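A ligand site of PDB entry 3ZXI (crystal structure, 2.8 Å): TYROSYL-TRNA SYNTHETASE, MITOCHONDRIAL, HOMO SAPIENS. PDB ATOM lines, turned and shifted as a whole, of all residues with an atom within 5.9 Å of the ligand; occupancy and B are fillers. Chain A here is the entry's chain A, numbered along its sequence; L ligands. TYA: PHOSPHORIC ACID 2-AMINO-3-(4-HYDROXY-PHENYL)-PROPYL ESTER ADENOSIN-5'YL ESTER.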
ATOM      1  N   TYR A  50     -15.772  20.332  38.734  1.00  0.00           N
ATOM      2  CA  TYR A  50     -16.358  21.435  37.969  1.00  0.00           C
ATOM      3  C   TYR A  50     -15.737  21.683  36.616  1.00  0.00           C
ATOM      4  O   TYR A  50     -14.585  21.328  36.363  1.00  0.00           O
ATOM      5  CB  TYR A  50     -16.420  22.735  38.784  1.00  0.00           C
ATOM      6  CG  TYR A  50     -15.271  23.719  38.585  1.00  0.00           C
ATOM      7  CD1 TYR A  50     -15.344  24.726  37.619  1.00  0.00           C
ATOM      8  CD2 TYR A  50     -14.145  23.670  39.399  1.00  0.00           C
ATOM      9  CE1 TYR A  50     -14.305  25.657  37.456  1.00  0.00           C
ATOM     10  CE2 TYR A  50     -13.104  24.599  39.246  1.00  0.00           C
ATOM     11  CZ  TYR A  50     -13.191  25.580  38.270  1.00  0.00           C
ATOM     12  OH  TYR A  50     -12.158  26.480  38.125  1.00  0.00           O
ATOM     13  N   CYS A  51     -16.524  22.298  35.742  1.00  0.00           N
ATOM     14  CA  CYS A  51     -16.064  22.730  34.434  1.00  0.00           C
ATOM     15  C   CYS A  51     -16.799  24.002  34.045  1.00  0.00           C
ATOM     16  O   CYS A  51     -18.023  24.107  34.250  1.00  0.00           O
ATOM     17  CB  CYS A  51     -16.329  21.634  33.399  1.00  0.00           C
ATOM     18  SG  CYS A  51     -16.091  22.167  31.677  1.00  0.00           S
ATOM     19  N   GLY A  52     -16.061  24.958  33.491  1.00  0.00           N
ATOM     20  CA  GLY A  52     -16.604  26.249  33.110  1.00  0.00           C
ATOM     21  C   GLY A  52     -16.899  26.399  31.628  1.00  0.00           C
ATOM     22  O   GLY A  52     -16.244  25.798  30.771  1.00  0.00           O
ATOM     23  N   PHE A  53     -17.883  27.219  31.330  1.00  0.00           N
ATOM     24  CA  PHE A  53     -18.332  27.407  29.974  1.00  0.00           C
ATOM     25  C   PHE A  53     -18.543  28.882  29.743  1.00  0.00           C
ATOM     26  O   PHE A  53     -19.493  29.472  30.265  1.00  0.00           O
ATOM     27  CB  PHE A  53     -19.664  26.671  29.770  1.00  0.00           C
ATOM     28  CG  PHE A  53     -19.605  25.233  30.074  1.00  0.00           C
ATOM     29  CD1 PHE A  53     -19.724  24.782  31.372  1.00  0.00           C
ATOM     30  CD2 PHE A  53     -19.405  24.315  29.063  1.00  0.00           C
ATOM     31  CE1 PHE A  53     -19.658  23.429  31.665  1.00  0.00           C
ATOM     32  CE2 PHE A  53     -19.331  22.970  29.335  1.00  0.00           C
ATOM     33  CZ  PHE A  53     -19.456  22.532  30.636  1.00  0.00           C
ATOM     34  N   ASP A  54     -17.654  29.502  28.977  1.00  0.00           N
ATOM     35  CA  ASP A  54     -17.737  30.956  28.777  1.00  0.00           C
ATOM     36  C   ASP A  54     -18.867  31.357  27.848  1.00  0.00           C
ATOM     37  O   ASP A  54     -18.981  30.872  26.713  1.00  0.00           O
ATOM     38  CB  ASP A  54     -16.411  31.521  28.273  1.00  0.00           C
ATOM     39  CG  ASP A  54     -15.672  32.280  29.356  1.00  0.00           C
ATOM     40  OD1 ASP A  54     -16.096  32.205  30.528  1.00  0.00           O
ATOM     41  OD2 ASP A  54     -14.664  32.927  29.012  1.00  0.00           O
ATOM     42  N   PRO A  55     -19.745  32.231  28.350  1.00  0.00           N
ATOM     43  CA  PRO A  55     -20.937  32.704  27.641  1.00  0.00           C
ATOM     44  C   PRO A  55     -20.588  33.714  26.580  1.00  0.00           C
ATOM     45  O   PRO A  55     -21.145  34.785  26.560  1.00  0.00           O
ATOM     46  CB  PRO A  55     -21.758  33.355  28.735  1.00  0.00           C
ATOM     47  CG  PRO A  55     -20.757  33.795  29.734  1.00  0.00           C
ATOM     48  CD  PRO A  55     -19.691  32.733  29.739  1.00  0.00           C
ATOM     49  N   THR A  56     -19.665  33.362  25.689  1.00  0.00           N
ATOM     50  CA  THR A  56     -19.312  34.210  24.570  1.00  0.00           C
ATOM     51  C   THR A  56     -20.321  34.069  23.439  1.00  0.00           C
ATOM     52  O   THR A  56     -20.191  34.703  22.409  1.00  0.00           O
ATOM     53  CB  THR A  56     -17.904  33.887  24.045  1.00  0.00           C
ATOM     54  OG1 THR A  56     -17.860  32.543  23.545  1.00  0.00           O
ATOM     55  CG2 THR A  56     -16.865  34.092  25.155  1.00  0.00           C
ATOM     56  N   HIS A  61     -22.310  24.484  21.966  1.00  0.00           N
ATOM     57  CA  HIS A  61     -22.173  23.672  20.758  1.00  0.00           C
ATOM     58  C   HIS A  61     -21.615  22.291  21.058  1.00  0.00           C
ATOM     59  O   HIS A  61     -21.157  22.009  22.165  1.00  0.00           O
ATOM     60  CB  HIS A  61     -21.272  24.369  19.747  1.00  0.00           C
ATOM     61  CG  HIS A  61     -19.867  24.571  20.240  1.00  0.00           C
ATOM     62  ND1 HIS A  61     -19.107  23.535  20.721  1.00  0.00           N
ATOM     63  CD2 HIS A  61     -19.111  25.686  20.349  1.00  0.00           C
ATOM     64  CE1 HIS A  61     -17.921  24.002  21.098  1.00  0.00           C
ATOM     65  NE2 HIS A  61     -17.911  25.300  20.889  1.00  0.00           N
ATOM     66  N   VAL A  62     -21.633  21.441  20.028  1.00  0.00           N
ATOM     67  CA  VAL A  62     -21.232  20.031  20.149  1.00  0.00           C
ATOM     68  C   VAL A  62     -19.902  19.771  20.880  1.00  0.00           C
ATOM     69  O   VAL A  62     -19.747  18.749  21.556  1.00  0.00           O
ATOM     70  CB  VAL A  62     -21.186  19.380  18.760  1.00  0.00           C
ATOM     71  CG1 VAL A  62     -20.505  18.052  18.841  1.00  0.00           C
ATOM     72  CG2 VAL A  62     -22.586  19.243  18.212  1.00  0.00           C
ATOM     73  N   GLY A  63     -18.940  20.678  20.748  1.00  0.00           N
ATOM     74  CA  GLY A  63     -17.716  20.569  21.491  1.00  0.00           C
ATOM     75  C   GLY A  63     -17.949  20.710  22.986  1.00  0.00           C
ATOM     76  O   GLY A  63     -17.399  19.945  23.782  1.00  0.00           O
ATOM     77  N   HIS A  64     -18.754  21.698  23.377  1.00  0.00           N
ATOM     78  CA  HIS A  64     -19.080  21.911  24.784  1.00  0.00           C
ATOM     79  C   HIS A  64     -19.674  20.637  25.331  1.00  0.00           C
ATOM     80  O   HIS A  64     -19.484  20.269  26.485  1.00  0.00           O
ATOM     81  CB  HIS A  64     -20.077  23.059  24.941  1.00  0.00           C
ATOM     82  CG  HIS A  64     -19.562  24.365  24.422  1.00  0.00           C
ATOM     83  ND1 HIS A  64     -18.249  24.744  24.559  1.00  0.00           N
ATOM     84  CD2 HIS A  64     -20.172  25.336  23.707  1.00  0.00           C
ATOM     85  CE1 HIS A  64     -18.067  25.906  23.971  1.00  0.00           C
ATOM     86  NE2 HIS A  64     -19.218  26.294  23.437  1.00  0.00           N
ATOM     87  N   LEU A  66     -19.036  17.592  24.829  1.00  0.00           N
ATOM     88  CA  LEU A  66     -18.036  16.641  25.313  1.00  0.00           C
ATOM     89  C   LEU A  66     -17.623  16.909  26.759  1.00  0.00           C
ATOM     90  O   LEU A  66     -17.609  15.994  27.588  1.00  0.00           O
ATOM     91  CB  LEU A  66     -16.799  16.648  24.393  1.00  0.00           C
ATOM     92  CG  LEU A  66     -16.089  15.325  24.234  1.00  0.00           C
ATOM     93  CD1 LEU A  66     -17.125  14.228  24.117  1.00  0.00           C
ATOM     94  CD2 LEU A  66     -15.174  15.341  23.010  1.00  0.00           C
ATOM     95  N   ALA A  67     -17.285  18.156  27.077  1.00  0.00           N
ATOM     96  CA  ALA A  67     -16.838  18.488  28.417  1.00  0.00           C
ATOM     97  C   ALA A  67     -17.966  18.273  29.399  1.00  0.00           C
ATOM     98  O   ALA A  67     -17.741  17.795  30.516  1.00  0.00           O
ATOM     99  CB  ALA A  67     -16.392  19.882  28.460  1.00  0.00           C
ATOM    100  N   LEU A  84     -20.193  25.593  35.592  1.00  0.00           N
ATOM    101  CA  LEU A  84     -20.027  27.020  35.861  1.00  0.00           C
ATOM    102  C   LEU A  84     -20.178  27.904  34.626  1.00  0.00           C
ATOM    103  O   LEU A  84     -19.524  27.654  33.600  1.00  0.00           O
ATOM    104  CB  LEU A  84     -18.655  27.265  36.466  1.00  0.00           C
ATOM    105  CG  LEU A  84     -18.348  28.717  36.877  1.00  0.00           C
ATOM    106  CD1 LEU A  84     -19.383  29.198  37.883  1.00  0.00           C
ATOM    107  CD2 LEU A  84     -16.958  28.923  37.449  1.00  0.00           C
ATOM    108  N   VAL A  85     -21.013  28.945  34.717  1.00  0.00           N
ATOM    109  CA  VAL A  85     -21.061  29.955  33.660  1.00  0.00           C
ATOM    110  C   VAL A  85     -20.042  31.121  33.876  1.00  0.00           C
ATOM    111  O   VAL A  85     -19.909  31.674  34.985  1.00  0.00           O
ATOM    112  CB  VAL A  85     -22.498  30.494  33.424  1.00  0.00           C
ATOM    113  CG1 VAL A  85     -22.480  31.648  32.421  1.00  0.00           C
ATOM    114  CG2 VAL A  85     -23.405  29.387  32.920  1.00  0.00           C
ATOM    115  N   GLY A  86     -19.314  31.479  32.824  1.00  0.00           N
ATOM    116  CA  GLY A  86     -18.285  32.493  32.951  1.00  0.00           C
ATOM    117  C   GLY A  86     -18.774  33.900  32.655  1.00  0.00           C
ATOM    118  O   GLY A  86     -18.273  34.563  31.739  1.00  0.00           O
ATOM    119  N   THR A  89     -15.674  36.162  33.243  1.00  0.00           N
ATOM    120  CA  THR A  89     -14.561  35.830  32.351  1.00  0.00           C
ATOM    121  C   THR A  89     -14.820  35.965  30.856  1.00  0.00           C
ATOM    122  O   THR A  89     -13.876  36.065  30.091  1.00  0.00           O
ATOM    123  CB  THR A  89     -14.056  34.406  32.618  1.00  0.00           C
ATOM    124  OG1 THR A  89     -15.169  33.525  32.863  1.00  0.00           O
ATOM    125  CG2 THR A  89     -13.108  34.386  33.817  1.00  0.00           C
ATOM    126  N   ASP A  94     -11.135  34.021  26.794  1.00  0.00           N
ATOM    127  CA  ASP A  94     -10.012  33.083  26.948  1.00  0.00           C
ATOM    128  C   ASP A  94      -8.996  33.218  25.807  1.00  0.00           C
ATOM    129  O   ASP A  94      -9.335  33.064  24.631  1.00  0.00           O
ATOM    130  CB  ASP A  94     -10.503  31.628  27.035  1.00  0.00           C
ATOM    131  CG  ASP A  94      -9.529  30.713  27.786  1.00  0.00           C
ATOM    132  OD1 ASP A  94      -8.334  31.044  27.867  1.00  0.00           O
ATOM    133  OD2 ASP A  94      -9.984  29.653  28.292  1.00  0.00           O
ATOM    134  N   ASN A 146     -19.663  32.779  37.936  1.00  0.00           N
ATOM    135  CA  ASN A 146     -18.583  33.530  38.620  1.00  0.00           C
ATOM    136  C   ASN A 146     -18.816  35.025  38.778  1.00  0.00           C
ATOM    137  O   ASN A 146     -18.188  35.664  39.624  1.00  0.00           O
ATOM    138  CB  ASN A 146     -17.194  33.271  38.004  1.00  0.00           C
ATOM    139  CG  ASN A 146     -17.180  33.383  36.476  1.00  0.00           C
ATOM    140  OD1 ASN A 146     -18.057  34.006  35.874  1.00  0.00           O
ATOM    141  ND2 ASN A 146     -16.161  32.768  35.855  1.00  0.00           N
ATOM    142  N   TYR A 194      -6.642  36.907  32.405  1.00  0.00           N
ATOM    143  CA  TYR A 194      -7.647  35.851  32.296  1.00  0.00           C
ATOM    144  C   TYR A 194      -7.308  34.610  33.094  1.00  0.00           C
ATOM    145  O   TYR A 194      -8.130  34.157  33.897  1.00  0.00           O
ATOM    146  CB  TYR A 194      -7.819  35.453  30.843  1.00  0.00           C
ATOM    147  CG  TYR A 194      -9.042  34.617  30.643  1.00  0.00           C
ATOM    148  CD1 TYR A 194      -9.041  33.279  30.990  1.00  0.00           C
ATOM    149  CD2 TYR A 194     -10.201  35.169  30.125  1.00  0.00           C
ATOM    150  CE1 TYR A 194     -10.180  32.506  30.827  1.00  0.00           C
ATOM    151  CE2 TYR A 194     -11.343  34.398  29.952  1.00  0.00           C
ATOM    152  CZ  TYR A 194     -11.338  33.068  30.300  1.00  0.00           C
ATOM    153  OH  TYR A 194     -12.468  32.302  30.124  1.00  0.00           O
ATOM    154  N   LEU A 197      -8.029  34.778  36.946  1.00  0.00           N
ATOM    155  CA  LEU A 197      -9.405  34.593  37.396  1.00  0.00           C
ATOM    156  C   LEU A 197      -9.784  33.103  37.487  1.00  0.00           C
ATOM    157  O   LEU A 197     -10.181  32.619  38.557  1.00  0.00           O
ATOM    158  CB  LEU A 197     -10.379  35.318  36.448  1.00  0.00           C
ATOM    159  CG  LEU A 197      -9.862  36.694  36.108  1.00  0.00           C
ATOM    160  CD1 LEU A 197     -10.765  37.392  35.103  1.00  0.00           C
ATOM    161  CD2 LEU A 197      -9.816  37.429  37.408  1.00  0.00           C
ATOM    162  N   GLN A 198      -9.667  32.383  36.373  1.00  0.00           N
ATOM    163  CA  GLN A 198      -9.933  30.936  36.352  1.00  0.00           C
ATOM    164  C   GLN A 198      -9.219  30.236  37.498  1.00  0.00           C
ATOM    165  O   GLN A 198      -9.783  29.336  38.123  1.00  0.00           O
ATOM    166  CB  GLN A 198      -9.536  30.336  35.002  1.00  0.00           C
ATOM    167  CG  GLN A 198      -9.715  28.834  34.904  1.00  0.00           C
ATOM    168  CD  GLN A 198     -10.009  28.366  33.477  1.00  0.00           C
ATOM    169  OE1 GLN A 198     -10.250  29.169  32.583  1.00  0.00           O
ATOM    170  NE2 GLN A 198     -10.012  27.054  33.281  1.00  0.00           N
ATOM    171  N   ASP A 201     -11.265  31.181  40.567  1.00  0.00           N
ATOM    172  CA  ASP A 201     -12.496  30.366  40.573  1.00  0.00           C
ATOM    173  C   ASP A 201     -12.312  28.997  41.241  1.00  0.00           C
ATOM    174  O   ASP A 201     -12.986  28.662  42.227  1.00  0.00           O
ATOM    175  CB  ASP A 201     -13.022  30.165  39.150  1.00  0.00           C
ATOM    176  CG  ASP A 201     -13.515  31.453  38.532  1.00  0.00           C
ATOM    177  OD1 ASP A 201     -13.590  32.446  39.274  1.00  0.00           O
ATOM    178  OD2 ASP A 201     -13.843  31.468  37.325  1.00  0.00           O
ATOM    179  N   PHE A 202     -11.411  28.202  40.681  1.00  0.00           N
ATOM    180  CA  PHE A 202     -11.051  26.905  41.253  1.00  0.00           C
ATOM    181  C   PHE A 202     -10.778  27.055  42.755  1.00  0.00           C
ATOM    182  O   PHE A 202     -11.132  26.184  43.554  1.00  0.00           O
ATOM    183  CB  PHE A 202      -9.826  26.338  40.524  1.00  0.00           C
ATOM    184  CG  PHE A 202      -9.633  24.851  40.686  1.00  0.00           C
ATOM    185  CD1 PHE A 202     -10.468  24.099  41.500  1.00  0.00           C
ATOM    186  CD2 PHE A 202      -8.603  24.200  40.014  1.00  0.00           C
ATOM    187  CE1 PHE A 202     -10.284  22.724  41.639  1.00  0.00           C
ATOM    188  CE2 PHE A 202      -8.418  22.835  40.144  1.00  0.00           C
ATOM    189  CZ  PHE A 202      -9.257  22.097  40.961  1.00  0.00           C
ATOM    190  N   GLN A 214     -11.127  19.929  38.709  1.00  0.00           N
ATOM    191  CA  GLN A 214     -11.611  20.718  37.601  1.00  0.00           C
ATOM    192  C   GLN A 214     -11.401  19.965  36.307  1.00  0.00           C
ATOM    193  O   GLN A 214     -10.384  19.296  36.121  1.00  0.00           O
ATOM    194  CB  GLN A 214     -10.889  22.068  37.513  1.00  0.00           C
ATOM    195  CG  GLN A 214     -11.411  22.939  36.366  1.00  0.00           C
ATOM    196  CD  GLN A 214     -10.743  24.299  36.305  1.00  0.00           C
ATOM    197  OE1 GLN A 214     -11.068  25.114  35.450  1.00  0.00           O
ATOM    198  NE2 GLN A 214      -9.805  24.551  37.211  1.00  0.00           N
ATOM    199  N   LEU A 215     -12.374  20.073  35.413  1.00  0.00           N
ATOM    200  CA  LEU A 215     -12.318  19.372  34.141  1.00  0.00           C
ATOM    201  C   LEU A 215     -12.679  20.317  33.009  1.00  0.00           C
ATOM    202  O   LEU A 215     -13.539  21.182  33.166  1.00  0.00           O
ATOM    203  CB  LEU A 215     -13.269  18.172  34.152  1.00  0.00           C
ATOM    204  CG  LEU A 215     -13.486  17.530  32.781  1.00  0.00           C
ATOM    205  CD1 LEU A 215     -13.511  16.004  32.886  1.00  0.00           C
ATOM    206  CD2 LEU A 215     -14.734  18.092  32.070  1.00  0.00           C
ATOM    207  N   GLY A 216     -12.025  20.146  31.868  1.00  0.00           N
ATOM    208  CA  GLY A 216     -12.312  20.955  30.683  1.00  0.00           C
ATOM    209  C   GLY A 216     -11.655  20.254  29.504  1.00  0.00           C
ATOM    210  O   GLY A 216     -11.094  19.167  29.678  1.00  0.00           O
ATOM    211  N   GLY A 217     -11.753  20.856  28.316  1.00  0.00           N
ATOM    212  CA  GLY A 217     -11.050  20.385  27.136  1.00  0.00           C
ATOM    213  C   GLY A 217      -9.540  20.400  27.369  1.00  0.00           C
ATOM    214  O   GLY A 217      -9.075  20.797  28.439  1.00  0.00           O
ATOM    215  N   SER A 218      -8.776  19.953  26.365  1.00  0.00           N
ATOM    216  CA  SER A 218      -7.326  19.930  26.505  1.00  0.00           C
ATOM    217  C   SER A 218      -6.737  21.334  26.433  1.00  0.00           C
ATOM    218  O   SER A 218      -5.756  21.639  27.112  1.00  0.00           O
ATOM    219  CB  SER A 218      -6.697  19.010  25.459  1.00  0.00           C
ATOM    220  OG  SER A 218      -7.519  18.934  24.303  1.00  0.00           O
ATOM    221  N   ASP A 219      -7.364  22.195  25.633  1.00  0.00           N
ATOM    222  CA  ASP A 219      -6.993  23.623  25.556  1.00  0.00           C
ATOM    223  C   ASP A 219      -6.953  24.348  26.909  1.00  0.00           C
ATOM    224  O   ASP A 219      -6.534  25.493  26.996  1.00  0.00           O
ATOM    225  CB  ASP A 219      -7.909  24.380  24.574  1.00  0.00           C
ATOM    226  CG  ASP A 219      -9.394  24.179  24.865  1.00  0.00           C
ATOM    227  OD1 ASP A 219      -9.793  23.057  25.249  1.00  0.00           O
ATOM    228  OD2 ASP A 219     -10.170  25.149  24.696  1.00  0.00           O
ATOM    229  N   GLN A 220      -7.378  23.661  27.968  1.00  0.00           N
ATOM    230  CA  GLN A 220      -7.538  24.274  29.269  1.00  0.00           C
ATOM    231  C   GLN A 220      -6.543  23.744  30.250  1.00  0.00           C
ATOM    232  O   GLN A 220      -6.658  24.017  31.455  1.00  0.00           O
ATOM    233  CB  GLN A 220      -8.947  23.992  29.798  1.00  0.00           C
ATOM    234  CG  GLN A 220     -10.058  24.555  28.931  1.00  0.00           C
ATOM    235  CD  GLN A 220     -10.044  26.063  28.910  1.00  0.00           C
ATOM    236  OE1 GLN A 220      -9.803  26.671  29.942  1.00  0.00           O
ATOM    237  NE2 GLN A 220     -10.270  26.662  27.749  1.00  0.00           N
ATOM    238  N   ASN A 223      -4.710  26.618  32.124  1.00  0.00           N
ATOM    239  CA  ASN A 223      -5.471  27.344  33.148  1.00  0.00           C
ATOM    240  C   ASN A 223      -5.646  26.538  34.430  1.00  0.00           C
ATOM    241  O   ASN A 223      -5.327  27.004  35.523  1.00  0.00           O
ATOM    242  CB  ASN A 223      -6.840  27.809  32.617  1.00  0.00           C
ATOM    243  CG  ASN A 223      -6.703  28.811  31.482  1.00  0.00           C
ATOM    244  OD1 ASN A 223      -5.658  29.447  31.315  1.00  0.00           O
ATOM    245  ND2 ASN A 223      -7.761  28.951  30.693  1.00  0.00           N
ATOM    246  N   VAL A 244     -10.236  16.278  28.479  1.00  0.00           N
ATOM    247  CA  VAL A 244     -10.999  15.469  27.543  1.00  0.00           C
ATOM    248  C   VAL A 244     -10.629  15.908  26.136  1.00  0.00           C
ATOM    249  O   VAL A 244     -10.253  17.046  25.920  1.00  0.00           O
ATOM    250  CB  VAL A 244     -12.510  15.648  27.751  1.00  0.00           C
ATOM    251  CG1 VAL A 244     -12.827  15.834  29.246  1.00  0.00           C
ATOM    252  CG2 VAL A 244     -13.030  16.823  26.934  1.00  0.00           C
ATOM    253  N   PRO A 245     -10.743  14.998  25.158  1.00  0.00           N
ATOM    254  CA  PRO A 245     -10.309  15.322  23.799  1.00  0.00           C
ATOM    255  C   PRO A 245     -11.052  16.528  23.181  1.00  0.00           C
ATOM    256  O   PRO A 245     -12.153  16.847  23.614  1.00  0.00           O
ATOM    257  CB  PRO A 245     -10.627  14.036  23.016  1.00  0.00           C
ATOM    258  CG  PRO A 245     -10.608  12.974  24.054  1.00  0.00           C
ATOM    259  CD  PRO A 245     -11.183  13.607  25.282  1.00  0.00           C
ATOM    260  N   LEU A 246     -10.447  17.162  22.176  1.00  0.00           N
ATOM    261  CA  LEU A 246     -11.074  18.207  21.393  1.00  0.00           C
ATOM    262  C   LEU A 246     -11.513  17.667  20.019  1.00  0.00           C
ATOM    263  O   LEU A 246     -10.703  17.086  19.287  1.00  0.00           O
ATOM    264  CB  LEU A 246     -10.097  19.380  21.201  1.00  0.00           C
ATOM    265  CG  LEU A 246      -9.699  20.199  22.438  1.00  0.00           C
ATOM    266  CD1 LEU A 246      -8.564  21.182  22.107  1.00  0.00           C
ATOM    267  CD2 LEU A 246     -10.887  20.925  23.095  1.00  0.00           C
ATOM    268  N   ILE A 247     -12.788  17.851  19.682  1.00  0.00           N
ATOM    269  CA  ILE A 247     -13.287  17.354  18.407  1.00  0.00           C
ATOM    270  C   ILE A 247     -13.289  18.411  17.300  1.00  0.00           C
ATOM    271  O   ILE A 247     -13.440  19.611  17.569  1.00  0.00           O
ATOM    272  CB  ILE A 247     -14.683  16.754  18.537  1.00  0.00           C
ATOM    273  CG1 ILE A 247     -15.662  17.833  18.973  1.00  0.00           C
ATOM    274  CG2 ILE A 247     -14.651  15.580  19.512  1.00  0.00           C
ATOM    275  CD1 ILE A 247     -16.948  17.283  19.542  1.00  0.00           C
ATOM    276  N   THR A 248     -13.138  17.941  16.066  1.00  0.00           N
ATOM    277  CA  THR A 248     -12.844  18.803  14.925  1.00  0.00           C
ATOM    278  C   THR A 248     -13.828  18.565  13.782  1.00  0.00           C
ATOM    279  O   THR A 248     -13.538  18.889  12.625  1.00  0.00           O
ATOM    280  CB  THR A 248     -11.418  18.558  14.427  1.00  0.00           C
ATOM    281  OG1 THR A 248     -11.438  17.679  13.298  1.00  0.00           O
ATOM    282  CG2 THR A 248     -10.554  17.948  15.542  1.00  0.00           C
HETATM  283  OPP TYA L   1     -13.391  27.795  27.351  1.00  0.00           O
HETATM  284  P   TYA L   1     -14.859  27.676  26.752  1.00  0.00           P
HETATM  285  O1P TYA L   1     -14.769  27.260  25.196  1.00  0.00           O
HETATM  286  O2P TYA L   1     -15.642  28.986  26.911  1.00  0.00           O
HETATM  287  O5' TYA L   1     -15.501  26.500  27.592  1.00  0.00           O
HETATM  288  C5' TYA L   1     -15.991  25.335  26.953  1.00  0.00           C
HETATM  289  C4' TYA L   1     -15.403  24.085  27.538  1.00  0.00           C
HETATM  290  O4' TYA L   1     -15.509  23.020  26.565  1.00  0.00           O
HETATM  291  C3' TYA L   1     -13.937  24.168  27.889  1.00  0.00           C
HETATM  292  O3' TYA L   1     -13.626  23.161  28.857  1.00  0.00           O
HETATM  293  C2' TYA L   1     -13.278  23.817  26.551  1.00  0.00           C
HETATM  294  O2' TYA L   1     -11.952  23.349  26.651  1.00  0.00           O
HETATM  295  C1' TYA L   1     -14.226  22.760  26.002  1.00  0.00           C
HETATM  296  N9  TYA L   1     -14.374  22.774  24.540  1.00  0.00           N
HETATM  297  C8  TYA L   1     -14.663  23.811  23.728  1.00  0.00           C
HETATM  298  N7  TYA L   1     -14.716  23.370  22.464  1.00  0.00           N
HETATM  299  C5  TYA L   1     -14.487  22.023  22.478  1.00  0.00           C
HETATM  300  C6  TYA L   1     -14.409  21.023  21.502  1.00  0.00           C
HETATM  301  N6  TYA L   1     -14.618  21.340  20.135  1.00  0.00           N
HETATM  302  N1  TYA L   1     -14.127  19.763  21.882  1.00  0.00           N
HETATM  303  C2  TYA L   1     -13.932  19.454  23.170  1.00  0.00           C
HETATM  304  N3  TYA L   1     -13.996  20.372  24.150  1.00  0.00           N
HETATM  305  C4  TYA L   1     -14.268  21.648  23.812  1.00  0.00           C
HETATM  306  NH2 TYA L   1     -11.984  28.781  30.378  1.00  0.00           N
HETATM  307  CA  TYA L   1     -13.171  28.203  29.742  1.00  0.00           C
HETATM  308  C   TYA L   1     -13.192  28.672  28.288  1.00  0.00           C
HETATM  309  CB  TYA L   1     -14.426  28.596  30.517  1.00  0.00           C
HETATM  310  CG  TYA L   1     -14.183  28.758  32.050  1.00  0.00           C
HETATM  311  CD1 TYA L   1     -14.642  29.889  32.707  1.00  0.00           C
HETATM  312  CD2 TYA L   1     -13.499  27.768  32.772  1.00  0.00           C
HETATM  313  CE1 TYA L   1     -14.418  30.020  34.062  1.00  0.00           C
HETATM  314  CE2 TYA L   1     -13.287  27.904  34.121  1.00  0.00           C
HETATM  315  CZ  TYA L   1     -13.742  29.044  34.778  1.00  0.00           C
HETATM  316  OH  TYA L   1     -13.541  29.195  36.112  1.00  0.00           O
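The backbone NH (N) of Ile 247 lies within hydrogen-bond range of a nitrogen (N1) of the ligand (3.2 Å).
A nitrogen (NH2) of the ligand lies within hydrogen-bond range of the side-chain amide oxygen (OE1) of Gln 198.
O2' of the ligand is in hydrogen-bond range of N of Gly 217, 3.0 Å away.
An oxygen (OH) of the ligand is in hydrogen-bond range of the side-chain carboxylate of Asp 201.
OE1 of Gln 220 lies within hydrogen-bond range of NH2 of the ligand (3.1 Å).
The side-chain carboxylate of Asp 94 lies within salt-bridge range of a nitrogen (NH2) of the ligand (3.0 Å).
O of Ile 247 sits at hydrogen-bond distance from N6 of the ligand, 3.3 Å away.
OD1 of Asp 219 is in hydrogen-bond range of O2' of the ligand (2.6 Å).
N of Asp 54 is in hydrogen-bond range of O2P of the ligand (2.9 Å).
The side-chain carboxylate (OD1) of Asp 54 sits at hydrogen-bond distance from the side-chain hydroxyl (OG1) of Thr 89.
The backbone carbonyl oxygen (O) of Phe 53 sits at hydrogen-bond distance from the backbone NH (N) of Gly 86 (3.3 Å).
The backbone NH (N) of Phe 202 lies within hydrogen-bond range of the side-chain hydroxyl (OH) of Tyr 50, 3.2 Å away.
O of Leu 84 sits at hydrogen-bond distance from N of Phe 53.
The backbone NH (N) of Gly 63 lies within hydrogen-bond range of a ring nitrogen (ND1) of His 61, 2.9 Å away.
The backbone carbonyl oxygen of Gly 216 is in hydrogen-bond range of the backbone NH of Val 244, at 3.2 Å.
The side-chain sulfur (SG) of Cys 51 sits close to the backbone carbonyl oxygen (O) of Leu 215 (3.1 Å).
The side-chain amide nitrogen (NE2) of Gln 198 is in hydrogen-bond range of the side-chain amide oxygen (OE1) of Gln 220 (3.4 Å).
An oxygen (O5') of the ligand lies close to the backbone carbonyl oxygen (O) of Gly 52 (3.3 Å).
A nitrogen (N3) of the ligand lies close to the backbone carbonyl oxygen of Gly 63 (3.4 Å).
OH of Tyr 50 touches OH of the ligand (3.7 Å).
Cys 51 touches the ligand (SG to O3', 3.9 Å).
Phe 53 touches the ligand (N to CB, 3.8 Å).
CE1 of His 61 touches N7 of the ligand, at 3.5 Å.
ND1 of His 64 touches C5' of the ligand (3.3 Å).
CB of Ala 67 touches O4' of the ligand, at 3.8 Å.
Leu 84 touches the ligand (CD2 to OH, 3.7 Å).
OG1 of Thr 89 touches CD1 of the ligand (3.7 Å).
Asn 146 touches the ligand.
Tyr 194 touches the ligand.
OE1 of Gln 214 touches CE2 of the ligand (3.8 Å).
Gly 216 touches the ligand.
O of Pro 245 touches C2 of the ligand (3.2 Å).
Leu 246 touches the ligand (CD2 to N3, 3.3 Å).
Hydrophobic or aromatic side chains that line the ligand: Tyr 50, His 61, His 64, Ala 67, Leu 84, Leu 246 and Ile 247.
24 residues have an atom within 4 Å of the ligand: Tyr 50, Cys 51, Gly 52, Phe 53, Asp 54, His 61, Gly 63, His 64, Ala 67, Leu 84, Thr 89, Asp 94, Asn 146, Tyr 194, Gln 198, Asp 201, Gln 214, Gly 216, Gly 217, Asp 219, Gln 220, Pro 245, Leu 246 and Ile 247.
The nearest printed residue that does not touch the ligand is Leu 66 (4.2 Å).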
